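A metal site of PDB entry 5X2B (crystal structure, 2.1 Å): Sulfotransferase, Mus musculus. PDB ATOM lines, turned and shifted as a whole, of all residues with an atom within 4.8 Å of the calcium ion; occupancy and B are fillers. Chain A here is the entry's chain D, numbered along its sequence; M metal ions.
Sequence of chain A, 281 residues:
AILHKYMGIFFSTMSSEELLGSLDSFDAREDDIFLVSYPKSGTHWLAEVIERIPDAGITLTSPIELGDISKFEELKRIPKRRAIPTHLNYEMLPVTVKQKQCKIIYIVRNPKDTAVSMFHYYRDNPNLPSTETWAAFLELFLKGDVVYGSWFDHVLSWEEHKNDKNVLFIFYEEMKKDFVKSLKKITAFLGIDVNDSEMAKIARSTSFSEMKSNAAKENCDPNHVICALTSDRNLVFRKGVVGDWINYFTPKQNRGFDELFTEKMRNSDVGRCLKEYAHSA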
ATOM      1  N   LYS A 162      18.299 -28.027 -13.580  1.00  0.00           N
ATOM      2  CA  LYS A 162      19.161 -27.518 -14.585  1.00  0.00           C
ATOM      3  C   LYS A 162      18.745 -28.094 -15.895  1.00  0.00           C
ATOM      4  O   LYS A 162      18.876 -27.459 -16.929  1.00  0.00           O
ATOM      5  CB  LYS A 162      20.593 -27.891 -14.321  1.00  0.00           C
ATOM      6  CG  LYS A 162      21.428 -27.649 -15.537  1.00  0.00           C
ATOM      7  CD  LYS A 162      22.796 -27.134 -15.233  1.00  0.00           C
ATOM      8  CE  LYS A 162      23.838 -27.819 -16.048  1.00  0.00           C
ATOM      9  NZ  LYS A 162      23.769 -27.445 -17.469  1.00  0.00           N
ATOM     10  N   ASN A 163      18.242 -29.308 -15.853  1.00  0.00           N
ATOM     11  CA  ASN A 163      17.709 -29.848 -17.066  1.00  0.00           C
ATOM     12  C   ASN A 163      16.393 -29.271 -17.323  1.00  0.00           C
ATOM     13  O   ASN A 163      15.766 -29.669 -18.280  1.00  0.00           O
ATOM     14  CB  ASN A 163      17.498 -31.341 -17.011  1.00  0.00           C
ATOM     15  CG  ASN A 163      18.769 -32.090 -16.975  1.00  0.00           C
ATOM     16  OD1 ASN A 163      19.777 -31.702 -17.580  1.00  0.00           O
ATOM     17  ND2 ASN A 163      18.745 -33.190 -16.272  1.00  0.00           N
ATOM     18  N   ASP A 164      15.933 -28.358 -16.480  1.00  0.00           N
ATOM     19  CA  ASP A 164      14.694 -27.695 -16.830  1.00  0.00           C
ATOM     20  C   ASP A 164      14.972 -26.749 -17.980  1.00  0.00           C
ATOM     21  O   ASP A 164      15.903 -25.937 -17.943  1.00  0.00           O
ATOM     22  CB  ASP A 164      14.102 -26.973 -15.660  1.00  0.00           C
ATOM     23  CG  ASP A 164      13.954 -27.819 -14.485  1.00  0.00           C
ATOM     24  OD1 ASP A 164      14.635 -28.873 -14.397  1.00  0.00           O
ATOM     25  OD2 ASP A 164      13.184 -27.411 -13.627  1.00  0.00           O
ATOM     26  N   LYS A 165      14.119 -26.865 -18.987  1.00  0.00           N
ATOM     27  CA  LYS A 165      14.274 -26.185 -20.276  1.00  0.00           C
ATOM     28  C   LYS A 165      14.365 -24.684 -20.127  1.00  0.00           C
ATOM     29  O   LYS A 165      15.127 -24.042 -20.827  1.00  0.00           O
ATOM     30  CB  LYS A 165      13.069 -26.497 -21.166  1.00  0.00           C
ATOM     31  CG  LYS A 165      11.849 -25.564 -20.999  1.00  0.00           C
ATOM     32  CD  LYS A 165      10.547 -26.352 -20.779  1.00  0.00           C
ATOM     33  CE  LYS A 165       9.611 -26.361 -21.990  1.00  0.00           C
ATOM     34  NZ  LYS A 165       8.663 -25.186 -21.980  1.00  0.00           N
ATOM     35  N   VAL A 167      15.543 -23.410 -17.695  1.00  0.00           N
ATOM     36  CA  VAL A 167      16.660 -23.106 -16.834  1.00  0.00           C
ATOM     37  C   VAL A 167      18.026 -23.233 -17.493  1.00  0.00           C
ATOM     38  O   VAL A 167      18.353 -24.283 -18.010  1.00  0.00           O
ATOM     39  CB  VAL A 167      16.718 -24.002 -15.669  1.00  0.00           C
ATOM     40  CG1 VAL A 167      17.967 -23.661 -14.853  1.00  0.00           C
ATOM     41  CG2 VAL A 167      15.528 -23.816 -14.836  1.00  0.00           C
ATOM     42  N   LEU A 168      18.840 -22.177 -17.379  1.00  0.00           N
ATOM     43  CA  LEU A 168      20.171 -22.162 -17.980  1.00  0.00           C
ATOM     44  C   LEU A 168      21.303 -21.838 -17.014  1.00  0.00           C
ATOM     45  O   LEU A 168      21.299 -20.823 -16.333  1.00  0.00           O
ATOM     46  CB  LEU A 168      20.242 -21.143 -19.127  1.00  0.00           C
ATOM     47  CG  LEU A 168      21.638 -20.826 -19.680  1.00  0.00           C
ATOM     48  CD1 LEU A 168      22.148 -21.877 -20.640  1.00  0.00           C
ATOM     49  CD2 LEU A 168      21.592 -19.479 -20.365  1.00  0.00           C
HETATM   50 CA    CA M   1      18.356 -26.104 -18.815  1.00  0.00          CA
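The calcium ion is bound by the backbone carbonyl oxygen of Val 167 (2.0 Å), the backbone carbonyl oxygen of Lys 162 (2.4 Å) and the backbone carbonyl oxygen of Asp 164 (2.6 Å).
The calcium ion has three donor atoms within binding distance.
Of the 6 residues printed, 3 come within 4 Å of the calcium ion.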
